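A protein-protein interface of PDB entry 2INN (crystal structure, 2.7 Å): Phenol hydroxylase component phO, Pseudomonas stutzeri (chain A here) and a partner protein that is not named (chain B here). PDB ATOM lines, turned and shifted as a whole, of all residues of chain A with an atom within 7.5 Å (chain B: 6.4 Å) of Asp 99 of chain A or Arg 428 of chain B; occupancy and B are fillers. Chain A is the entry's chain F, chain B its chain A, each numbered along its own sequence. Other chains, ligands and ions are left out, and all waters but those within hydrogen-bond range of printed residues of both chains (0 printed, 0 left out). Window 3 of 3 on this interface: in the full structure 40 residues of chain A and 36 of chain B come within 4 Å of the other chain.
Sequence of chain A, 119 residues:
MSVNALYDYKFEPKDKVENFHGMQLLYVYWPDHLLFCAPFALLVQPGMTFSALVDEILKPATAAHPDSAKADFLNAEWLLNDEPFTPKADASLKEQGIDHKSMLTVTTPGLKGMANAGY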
ATOM      1  N   ASP A  15      24.001  11.045 -27.021  1.00  0.00           N
ATOM      2  CA  ASP A  15      23.443   9.977 -27.791  1.00  0.00           C
ATOM      3  C   ASP A  15      22.197  10.356 -28.647  1.00  0.00           C
ATOM      4  O   ASP A  15      21.272   9.537 -28.775  1.00  0.00           O
ATOM      5  CB  ASP A  15      23.154   8.778 -26.882  1.00  0.00           C
ATOM      6  CG  ASP A  15      24.445   8.191 -26.237  1.00  0.00           C
ATOM      7  OD1 ASP A  15      24.343   7.435 -25.221  1.00  0.00           O
ATOM      8  OD2 ASP A  15      25.552   8.554 -26.723  1.00  0.00           O
ATOM      9  N   VAL A  17      19.987  10.602 -31.825  1.00  0.00           N
ATOM     10  CA  VAL A  17      20.015   9.771 -33.030  1.00  0.00           C
ATOM     11  C   VAL A  17      20.910  10.388 -34.178  1.00  0.00           C
ATOM     12  O   VAL A  17      21.516   9.656 -35.001  1.00  0.00           O
ATOM     13  CB  VAL A  17      18.586   9.395 -33.443  1.00  0.00           C
ATOM     14  CG1 VAL A  17      17.893  10.609 -34.134  1.00  0.00           C
ATOM     15  CG2 VAL A  17      18.603   8.167 -34.301  1.00  0.00           C
ATOM     16  N   GLN A  24      20.189   3.959 -35.975  1.00  0.00           N
ATOM     17  CA  GLN A  24      19.477   4.037 -34.751  1.00  0.00           C
ATOM     18  C   GLN A  24      20.060   2.980 -33.676  1.00  0.00           C
ATOM     19  O   GLN A  24      20.824   2.078 -34.040  1.00  0.00           O
ATOM     20  CB  GLN A  24      18.087   3.714 -35.195  1.00  0.00           C
ATOM     21  CG  GLN A  24      17.097   3.498 -34.114  1.00  0.00           C
ATOM     22  CD  GLN A  24      15.762   2.999 -34.653  1.00  0.00           C
ATOM     23  OE1 GLN A  24      15.103   3.622 -35.549  1.00  0.00           O
ATOM     24  NE2 GLN A  24      15.312   1.889 -34.060  1.00  0.00           N
ATOM     25  N   LEU A  25      19.755   3.100 -32.376  1.00  0.00           N
ATOM     26  CA  LEU A  25      20.113   2.083 -31.387  1.00  0.00           C
ATOM     27  C   LEU A  25      18.840   1.374 -31.038  1.00  0.00           C
ATOM     28  O   LEU A  25      17.829   2.004 -30.956  1.00  0.00           O
ATOM     29  CB  LEU A  25      20.637   2.670 -30.087  1.00  0.00           C
ATOM     30  CG  LEU A  25      22.068   3.189 -30.007  1.00  0.00           C
ATOM     31  CD1 LEU A  25      22.239   4.168 -28.826  1.00  0.00           C
ATOM     32  CD2 LEU A  25      23.037   2.044 -29.862  1.00  0.00           C
ATOM     33  N   LEU A  26      18.927   0.066 -30.780  1.00  0.00           N
ATOM     34  CA  LEU A  26      17.854  -0.736 -30.266  1.00  0.00           C
ATOM     35  C   LEU A  26      18.292  -1.617 -29.034  1.00  0.00           C
ATOM     36  O   LEU A  26      19.393  -2.220 -29.045  1.00  0.00           O
ATOM     37  CB  LEU A  26      17.478  -1.663 -31.370  1.00  0.00           C
ATOM     38  CG  LEU A  26      16.006  -1.932 -31.440  1.00  0.00           C
ATOM     39  CD1 LEU A  26      15.816  -3.319 -32.092  1.00  0.00           C
ATOM     40  CD2 LEU A  26      15.385  -1.874 -30.089  1.00  0.00           C
ATOM     41  N   TYR A  27      17.453  -1.752 -27.999  1.00  0.00           N
ATOM     42  CA  TYR A  27      17.710  -2.773 -27.033  1.00  0.00           C
ATOM     43  C   TYR A  27      16.744  -3.998 -27.178  1.00  0.00           C
ATOM     44  O   TYR A  27      15.543  -3.872 -27.539  1.00  0.00           O
ATOM     45  CB  TYR A  27      17.793  -2.168 -25.634  1.00  0.00           C
ATOM     46  CG  TYR A  27      18.787  -1.028 -25.567  1.00  0.00           C
ATOM     47  CD1 TYR A  27      20.190  -1.243 -25.706  1.00  0.00           C
ATOM     48  CD2 TYR A  27      18.340   0.301 -25.392  1.00  0.00           C
ATOM     49  CE1 TYR A  27      21.102  -0.130 -25.632  1.00  0.00           C
ATOM     50  CE2 TYR A  27      19.236   1.411 -25.352  1.00  0.00           C
ATOM     51  CZ  TYR A  27      20.598   1.181 -25.463  1.00  0.00           C
ATOM     52  OH  TYR A  27      21.417   2.285 -25.424  1.00  0.00           O
ATOM     53  N   PRO A  46      16.792   2.072 -39.265  1.00  0.00           N
ATOM     54  CA  PRO A  46      15.361   2.415 -38.994  1.00  0.00           C
ATOM     55  C   PRO A  46      14.355   1.723 -39.954  1.00  0.00           C
ATOM     56  O   PRO A  46      13.173   1.324 -39.568  1.00  0.00           O
ATOM     57  CB  PRO A  46      15.352   3.922 -39.215  1.00  0.00           C
ATOM     58  CG  PRO A  46      16.789   4.355 -38.754  1.00  0.00           C
ATOM     59  CD  PRO A  46      17.663   3.270 -39.333  1.00  0.00           C
ATOM     60  N   LEU A  80       7.285  -3.275 -26.053  1.00  0.00           N
ATOM     61  CA  LEU A  80       8.096  -2.178 -26.553  1.00  0.00           C
ATOM     62  C   LEU A  80       8.073  -1.259 -25.364  1.00  0.00           C
ATOM     63  O   LEU A  80       6.968  -0.757 -24.955  1.00  0.00           O
ATOM     64  CB  LEU A  80       7.423  -1.457 -27.739  1.00  0.00           C
ATOM     65  CG  LEU A  80       8.132  -0.725 -28.870  1.00  0.00           C
ATOM     66  CD1 LEU A  80       7.126   0.300 -29.516  1.00  0.00           C
ATOM     67  CD2 LEU A  80       9.454  -0.104 -28.483  1.00  0.00           C
ATOM     68  N   ASN A  81       9.255  -1.061 -24.777  1.00  0.00           N
ATOM     69  CA  ASN A  81       9.374  -0.020 -23.795  1.00  0.00           C
ATOM     70  C   ASN A  81       8.331  -0.243 -22.737  1.00  0.00           C
ATOM     71  O   ASN A  81       7.634   0.700 -22.370  1.00  0.00           O
ATOM     72  CB  ASN A  81       9.148   1.317 -24.482  1.00  0.00           C
ATOM     73  CG  ASN A  81      10.169   1.575 -25.465  1.00  0.00           C
ATOM     74  OD1 ASN A  81      11.062   0.814 -25.568  1.00  0.00           O
ATOM     75  ND2 ASN A  81      10.086   2.622 -26.192  1.00  0.00           N
ATOM     76  N   LEU A  93      10.989  -0.742 -38.851  1.00  0.00           N
ATOM     77  CA  LEU A  93      11.064  -0.563 -37.424  1.00  0.00           C
ATOM     78  C   LEU A  93      10.501   0.821 -37.222  1.00  0.00           C
ATOM     79  O   LEU A  93       9.528   0.975 -36.462  1.00  0.00           O
ATOM     80  CB  LEU A  93      12.530  -0.611 -36.982  1.00  0.00           C
ATOM     81  CG  LEU A  93      13.152  -1.913 -36.499  1.00  0.00           C
ATOM     82  CD1 LEU A  93      12.215  -3.092 -36.759  1.00  0.00           C
ATOM     83  CD2 LEU A  93      14.499  -2.114 -37.086  1.00  0.00           C
ATOM     84  N   LYS A  94      11.095   1.806 -37.930  1.00  0.00           N
ATOM     85  CA  LYS A  94      10.754   3.218 -37.729  1.00  0.00           C
ATOM     86  C   LYS A  94       9.272   3.349 -37.615  1.00  0.00           C
ATOM     87  O   LYS A  94       8.726   3.817 -36.594  1.00  0.00           O
ATOM     88  CB  LYS A  94      11.131   4.091 -38.923  1.00  0.00           C
ATOM     89  CG  LYS A  94      10.714   5.553 -38.689  1.00  0.00           C
ATOM     90  CD  LYS A  94      10.695   6.414 -39.967  1.00  0.00           C
ATOM     91  CE  LYS A  94      12.111   6.711 -40.501  1.00  0.00           C
ATOM     92  NZ  LYS A  94      12.718   7.796 -39.707  1.00  0.00           N
ATOM     93  N   GLU A  95       8.630   2.894 -38.683  1.00  0.00           N
ATOM     94  CA  GLU A  95       7.232   3.122 -38.851  1.00  0.00           C
ATOM     95  C   GLU A  95       6.395   2.421 -37.863  1.00  0.00           C
ATOM     96  O   GLU A  95       5.403   2.976 -37.506  1.00  0.00           O
ATOM     97  CB  GLU A  95       6.754   2.804 -40.257  1.00  0.00           C
ATOM     98  CG  GLU A  95       7.153   1.451 -40.823  1.00  0.00           C
ATOM     99  CD  GLU A  95       6.273   1.110 -42.015  1.00  0.00           C
ATOM    100  OE1 GLU A  95       6.769   0.663 -43.096  1.00  0.00           O
ATOM    101  OE2 GLU A  95       5.047   1.344 -41.829  1.00  0.00           O
ATOM    102  N   GLN A  96       6.726   1.234 -37.382  1.00  0.00           N
ATOM    103  CA  GLN A  96       5.851   0.776 -36.281  1.00  0.00           C
ATOM    104  C   GLN A  96       6.156   1.355 -34.885  1.00  0.00           C
ATOM    105  O   GLN A  96       5.721   0.788 -33.875  1.00  0.00           O
ATOM    106  CB  GLN A  96       5.691  -0.720 -36.205  1.00  0.00           C
ATOM    107  CG  GLN A  96       6.988  -1.431 -36.274  1.00  0.00           C
ATOM    108  CD  GLN A  96       6.776  -2.879 -36.576  1.00  0.00           C
ATOM    109  OE1 GLN A  96       7.296  -3.384 -37.567  1.00  0.00           O
ATOM    110  NE2 GLN A  96       5.953  -3.548 -35.759  1.00  0.00           N
ATOM    111  N   GLY A  97       6.880   2.469 -34.828  1.00  0.00           N
ATOM    112  CA  GLY A  97       7.154   3.086 -33.536  1.00  0.00           C
ATOM    113  C   GLY A  97       8.378   2.545 -32.764  1.00  0.00           C
ATOM    114  O   GLY A  97       8.521   2.814 -31.554  1.00  0.00           O
ATOM    115  N   ILE A  98       9.262   1.797 -33.464  1.00  0.00           N
ATOM    116  CA  ILE A  98      10.514   1.319 -32.876  1.00  0.00           C
ATOM    117  C   ILE A  98      11.670   2.310 -33.108  1.00  0.00           C
ATOM    118  O   ILE A  98      12.468   2.175 -34.050  1.00  0.00           O
ATOM    119  CB  ILE A  98      10.790  -0.077 -33.401  1.00  0.00           C
ATOM    120  CG1 ILE A  98       9.613  -0.959 -33.013  1.00  0.00           C
ATOM    121  CG2 ILE A  98      12.166  -0.622 -32.894  1.00  0.00           C
ATOM    122  CD1 ILE A  98       9.708  -2.355 -33.440  1.00  0.00           C
ATOM    123  N   ASP A  99      11.737   3.322 -32.242  1.00  0.00           N
ATOM    124  CA  ASP A  99      12.646   4.491 -32.457  1.00  0.00           C
ATOM    125  C   ASP A  99      14.008   4.381 -31.698  1.00  0.00           C
ATOM    126  O   ASP A  99      14.201   3.501 -30.858  1.00  0.00           O
ATOM    127  CB  ASP A  99      11.925   5.774 -32.037  1.00  0.00           C
ATOM    128  CG  ASP A  99      11.387   5.701 -30.576  1.00  0.00           C
ATOM    129  OD1 ASP A  99      11.880   4.904 -29.763  1.00  0.00           O
ATOM    130  OD2 ASP A  99      10.488   6.452 -30.194  1.00  0.00           O
ATOM    131  N   HIS A 100      14.940   5.286 -31.994  1.00  0.00           N
ATOM    132  CA  HIS A 100      16.259   5.317 -31.347  1.00  0.00           C
ATOM    133  C   HIS A 100      16.135   5.086 -29.876  1.00  0.00           C
ATOM    134  O   HIS A 100      15.328   5.684 -29.238  1.00  0.00           O
ATOM    135  CB  HIS A 100      16.839   6.667 -31.549  1.00  0.00           C
ATOM    136  CG  HIS A 100      18.181   6.854 -30.963  1.00  0.00           C
ATOM    137  ND1 HIS A 100      19.209   5.980 -31.186  1.00  0.00           N
ATOM    138  CD2 HIS A 100      18.715   7.884 -30.268  1.00  0.00           C
ATOM    139  CE1 HIS A 100      20.317   6.452 -30.640  1.00  0.00           C
ATOM    140  NE2 HIS A 100      20.042   7.599 -30.059  1.00  0.00           N
ATOM    141  N   LYS A 101      16.925   4.173 -29.353  1.00  0.00           N
ATOM    142  CA  LYS A 101      16.880   3.755 -27.967  1.00  0.00           C
ATOM    143  C   LYS A 101      15.629   3.124 -27.393  1.00  0.00           C
ATOM    144  O   LYS A 101      15.566   2.997 -26.157  1.00  0.00           O
ATOM    145  CB  LYS A 101      17.420   4.834 -27.057  1.00  0.00           C
ATOM    146  CG  LYS A 101      18.867   5.172 -27.353  1.00  0.00           C
ATOM    147  CD  LYS A 101      19.565   5.866 -26.175  1.00  0.00           C
ATOM    148  CE  LYS A 101      19.882   7.339 -26.420  1.00  0.00           C
ATOM    149  NZ  LYS A 101      19.539   8.059 -25.110  1.00  0.00           N
ATOM    150  N   SER A 102      14.661   2.683 -28.211  1.00  0.00           N
ATOM    151  CA  SER A 102      13.627   1.778 -27.620  1.00  0.00           C
ATOM    152  C   SER A 102      14.245   0.434 -27.280  1.00  0.00           C
ATOM    153  O   SER A 102      15.366   0.164 -27.616  1.00  0.00           O
ATOM    154  CB  SER A 102      12.338   1.525 -28.421  1.00  0.00           C
ATOM    155  OG  SER A 102      12.119   2.401 -29.491  1.00  0.00           O
ATOM    156  N   MET A 103      13.487  -0.353 -26.527  1.00  0.00           N
ATOM    157  CA  MET A 103      13.835  -1.698 -26.079  1.00  0.00           C
ATOM    158  C   MET A 103      12.659  -2.620 -26.269  1.00  0.00           C
ATOM    159  O   MET A 103      11.528  -2.356 -25.763  1.00  0.00           O
ATOM    160  CB  MET A 103      14.207  -1.754 -24.606  1.00  0.00           C
ATOM    161  CG  MET A 103      14.562  -3.216 -24.154  1.00  0.00           C
ATOM    162  SD  MET A 103      15.423  -3.510 -22.265  1.00  0.00           S
ATOM    163  CE  MET A 103      17.064  -2.335 -22.689  1.00  0.00           C
ATOM    164  N   GLN B 400      22.707   4.296 -17.895  1.00  0.00           N
ATOM    165  CA  GLN B 400      23.035   5.725 -18.081  1.00  0.00           C
ATOM    166  C   GLN B 400      23.736   6.309 -16.859  1.00  0.00           C
ATOM    167  O   GLN B 400      24.593   7.205 -16.976  1.00  0.00           O
ATOM    168  CB  GLN B 400      21.811   6.536 -18.385  1.00  0.00           C
ATOM    169  CG  GLN B 400      22.067   7.954 -18.893  1.00  0.00           C
ATOM    170  CD  GLN B 400      22.584   7.999 -20.331  1.00  0.00           C
ATOM    171  OE1 GLN B 400      23.497   8.808 -20.638  1.00  0.00           O
ATOM    172  NE2 GLN B 400      22.042   7.092 -21.220  1.00  0.00           N
ATOM    173  N   GLN B 421      13.568   2.453 -17.279  1.00  0.00           N
ATOM    174  CA  GLN B 421      13.556   3.172 -18.567  1.00  0.00           C
ATOM    175  C   GLN B 421      12.711   4.415 -18.431  1.00  0.00           C
ATOM    176  O   GLN B 421      11.584   4.347 -17.886  1.00  0.00           O
ATOM    177  CB  GLN B 421      12.866   2.259 -19.555  1.00  0.00           C
ATOM    178  CG  GLN B 421      12.584   2.850 -20.830  1.00  0.00           C
ATOM    179  CD  GLN B 421      12.333   1.833 -21.888  1.00  0.00           C
ATOM    180  OE1 GLN B 421      12.031   0.667 -21.629  1.00  0.00           O
ATOM    181  NE2 GLN B 421      12.497   2.259 -23.112  1.00  0.00           N
ATOM    182  N   ILE B 422      13.174   5.538 -18.945  1.00  0.00           N
ATOM    183  CA  ILE B 422      12.433   6.737 -18.685  1.00  0.00           C
ATOM    184  C   ILE B 422      12.435   7.529 -19.968  1.00  0.00           C
ATOM    185  O   ILE B 422      13.174   7.160 -20.911  1.00  0.00           O
ATOM    186  CB  ILE B 422      13.069   7.427 -17.457  1.00  0.00           C
ATOM    187  CG1 ILE B 422      12.061   8.287 -16.725  1.00  0.00           C
ATOM    188  CG2 ILE B 422      14.439   8.145 -17.738  1.00  0.00           C
ATOM    189  CD1 ILE B 422      12.780   9.416 -15.978  1.00  0.00           C
ATOM    190  N   GLU B 423      11.582   8.558 -20.112  1.00  0.00           N
ATOM    191  CA  GLU B 423      11.894   9.512 -21.225  1.00  0.00           C
ATOM    192  C   GLU B 423      12.239  10.845 -20.626  1.00  0.00           C
ATOM    193  O   GLU B 423      11.737  11.183 -19.597  1.00  0.00           O
ATOM    194  CB  GLU B 423      10.780   9.663 -22.253  1.00  0.00           C
ATOM    195  CG  GLU B 423       9.830   8.454 -22.316  1.00  0.00           C
ATOM    196  CD  GLU B 423       8.882   8.572 -23.476  1.00  0.00           C
ATOM    197  OE1 GLU B 423       9.342   8.865 -24.629  1.00  0.00           O
ATOM    198  OE2 GLU B 423       7.674   8.367 -23.211  1.00  0.00           O
ATOM    199  N   HIS B 424      13.107  11.577 -21.271  1.00  0.00           N
ATOM    200  CA  HIS B 424      13.366  12.872 -20.809  1.00  0.00           C
ATOM    201  C   HIS B 424      13.786  13.740 -21.976  1.00  0.00           C
ATOM    202  O   HIS B 424      14.772  13.404 -22.610  1.00  0.00           O
ATOM    203  CB  HIS B 424      14.420  12.823 -19.712  1.00  0.00           C
ATOM    204  CG  HIS B 424      14.982  14.165 -19.370  1.00  0.00           C
ATOM    205  ND1 HIS B 424      16.105  14.686 -20.005  1.00  0.00           N
ATOM    206  CD2 HIS B 424      14.553  15.118 -18.510  1.00  0.00           C
ATOM    207  CE1 HIS B 424      16.345  15.905 -19.538  1.00  0.00           C
ATOM    208  NE2 HIS B 424      15.396  16.201 -18.663  1.00  0.00           N
ATOM    209  N   GLY B 426      12.235  13.964 -24.828  1.00  0.00           N
ATOM    210  CA  GLY B 426      12.057  13.053 -26.015  1.00  0.00           C
ATOM    211  C   GLY B 426      13.333  12.263 -26.403  1.00  0.00           C
ATOM    212  O   GLY B 426      13.710  12.109 -27.593  1.00  0.00           O
ATOM    213  N   GLU B 427      14.044  11.858 -25.363  1.00  0.00           N
ATOM    214  CA  GLU B 427      15.194  11.017 -25.481  1.00  0.00           C
ATOM    215  C   GLU B 427      14.888  10.003 -24.434  1.00  0.00           C
ATOM    216  O   GLU B 427      14.332  10.318 -23.332  1.00  0.00           O
ATOM    217  CB  GLU B 427      16.440  11.817 -25.176  1.00  0.00           C
ATOM    218  CG  GLU B 427      16.624  12.846 -26.238  1.00  0.00           C
ATOM    219  CD  GLU B 427      17.275  12.235 -27.488  1.00  0.00           C
ATOM    220  OE1 GLU B 427      17.311  10.983 -27.649  1.00  0.00           O
ATOM    221  OE2 GLU B 427      17.800  13.010 -28.303  1.00  0.00           O
ATOM    222  N   ARG B 428      15.164   8.764 -24.818  1.00  0.00           N
ATOM    223  CA  ARG B 428      15.096   7.631 -23.855  1.00  0.00           C
ATOM    224  C   ARG B 428      16.413   7.287 -23.197  1.00  0.00           C
ATOM    225  O   ARG B 428      17.498   7.570 -23.699  1.00  0.00           O
ATOM    226  CB  ARG B 428      14.483   6.447 -24.537  1.00  0.00           C
ATOM    227  CG  ARG B 428      13.117   6.808 -25.293  1.00  0.00           C
ATOM    228  CD  ARG B 428      12.763   5.512 -25.985  1.00  0.00           C
ATOM    229  NE  ARG B 428      11.732   5.616 -26.960  1.00  0.00           N
ATOM    230  CZ  ARG B 428      10.426   5.518 -26.705  1.00  0.00           C
ATOM    231  NH1 ARG B 428       9.929   5.318 -25.444  1.00  0.00           N
ATOM    232  NH2 ARG B 428       9.611   5.664 -27.752  1.00  0.00           N
ATOM    233  N   TYR B 429      16.312   6.797 -21.988  1.00  0.00           N
ATOM    234  CA  TYR B 429      17.509   6.423 -21.254  1.00  0.00           C
ATOM    235  C   TYR B 429      17.125   5.261 -20.374  1.00  0.00           C
ATOM    236  O   TYR B 429      15.941   5.031 -20.039  1.00  0.00           O
ATOM    237  CB  TYR B 429      18.055   7.574 -20.424  1.00  0.00           C
ATOM    238  CG  TYR B 429      18.370   8.825 -21.203  1.00  0.00           C
ATOM    239  CD1 TYR B 429      19.632   9.005 -21.817  1.00  0.00           C
ATOM    240  CD2 TYR B 429      17.399   9.862 -21.317  1.00  0.00           C
ATOM    241  CE1 TYR B 429      19.943  10.179 -22.492  1.00  0.00           C
ATOM    242  CE2 TYR B 429      17.664  11.062 -21.997  1.00  0.00           C
ATOM    243  CZ  TYR B 429      18.939  11.211 -22.579  1.00  0.00           C
ATOM    244  OH  TYR B 429      19.194  12.375 -23.318  1.00  0.00           O
ATOM    245  N   HIS B 430      18.164   4.520 -20.040  1.00  0.00           N
ATOM    246  CA  HIS B 430      18.040   3.221 -19.447  1.00  0.00           C
ATOM    247  C   HIS B 430      18.930   3.097 -18.200  1.00  0.00           C
ATOM    248  O   HIS B 430      20.056   3.671 -18.132  1.00  0.00           O
ATOM    249  CB  HIS B 430      18.460   2.223 -20.525  1.00  0.00           C
ATOM    250  CG  HIS B 430      17.418   2.011 -21.592  1.00  0.00           C
ATOM    251  ND1 HIS B 430      16.390   1.088 -21.462  1.00  0.00           N
ATOM    252  CD2 HIS B 430      17.230   2.619 -22.794  1.00  0.00           C
ATOM    253  CE1 HIS B 430      15.630   1.127 -22.540  1.00  0.00           C
ATOM    254  NE2 HIS B 430      16.122   2.038 -23.366  1.00  0.00           N
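Printed residues of chain B within 4 Å of Asn 81 of chain A: Gln 421 and Arg 428. Lys 94 of chain A touches none of the printed residues of chain B. Asp 99 of chain A touches one residue of chain B. Printed residues of chain B within 4 Å of Lys 101 of chain A: Arg 428, Tyr 429 and His 430. Of the printed residues of chain B, Met 103 of chain A touches His 430. Of chain A, only Asn 81 (2.8 Å), Asp 99 (2.7 Å) and Lys 101 (2.5 Å) come within 4 Å of Arg 428 of chain B. Printed residues of chain A within 4 Å of Tyr 429 of chain B: Lys 101 (3.4 Å). Printed residues of chain A within 4 Å of His 430 of chain B: Tyr 27, Lys 101 and Met 103. The nearest printed residue of chain A that does not touch Tyr 429 of chain B is Asp 15 of chain A (5.6 Å).
Printed residues of chain B that touch a printed residue of chain A: Gln 421, Arg 428, Tyr 429 and His 430. Hydrophobic or aromatic side chains of chain B within 4 Å of the printed part of chain A: Tyr 429 and His 430. Among the printed residues, Asp or Glu carboxylates within 4 Å of a Lys or Arg side-chain nitrogen of the other chain: Asp 99 of chain A with Arg 428 of chain B (2.7 Å).
Among the printed residues, merely in contact across the chains: Tyr 27 of chain A with His 430 of chain B (3.5 Å), Lys 101 of chain A with Tyr 429 of chain B (3.4 Å) and Met 103 of chain A with His 430 of chain B (3.7 Å).
OD1 of Asn 81 of chain A is in hydrogen-bond range of NE2 of Gln 421 of chain B, at 3.2 Å. The guanidinium group (NH1) of Arg 428 of chain B sits close to the side-chain amide nitrogen (ND2) of Asn 81 of chain A (2.8 Å). The guanidinium group (NH2) of Arg 428 of chain B lies within salt-bridge range of the side-chain carboxylate (OD2) of Asp 99 of chain A. The backbone carbonyl oxygen (O) of Arg 428 of chain B is in hydrogen-bond range of the side-chain amino group (NZ) of Lys 101 of chain A. The backbone carbonyl oxygen (O) of Lys 101 of chain A sits at hydrogen-bond distance from a ring nitrogen (NE2) of His 430 of chain B, at 3.0 Å.
The backbone carbonyl oxygen of Tyr 429 of chain B is in hydrogen-bond range of the backbone NH of Ile 422 of chain B. NH1 of Arg 428 of chain B lies within salt-bridge range of OE1 of Glu 423 of chain B (3.7 Å). O of Leu 25 of chain A lies within hydrogen-bond range of N of Lys 101 of chain A (2.8 Å). The backbone NH (N) of Tyr 27 of chain A is in hydrogen-bond range of the backbone carbonyl oxygen (O) of Ser 102 of chain A, at 2.9 Å. The backbone NH (N) of Asn 81 of chain A lies within hydrogen-bond range of the backbone carbonyl oxygen (O) of Met 103 of chain A (2.8 Å). OD1 of Asp 99 of chain A sits at hydrogen-bond distance from OG of Ser 102 of chain A, 2.5 Å away.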
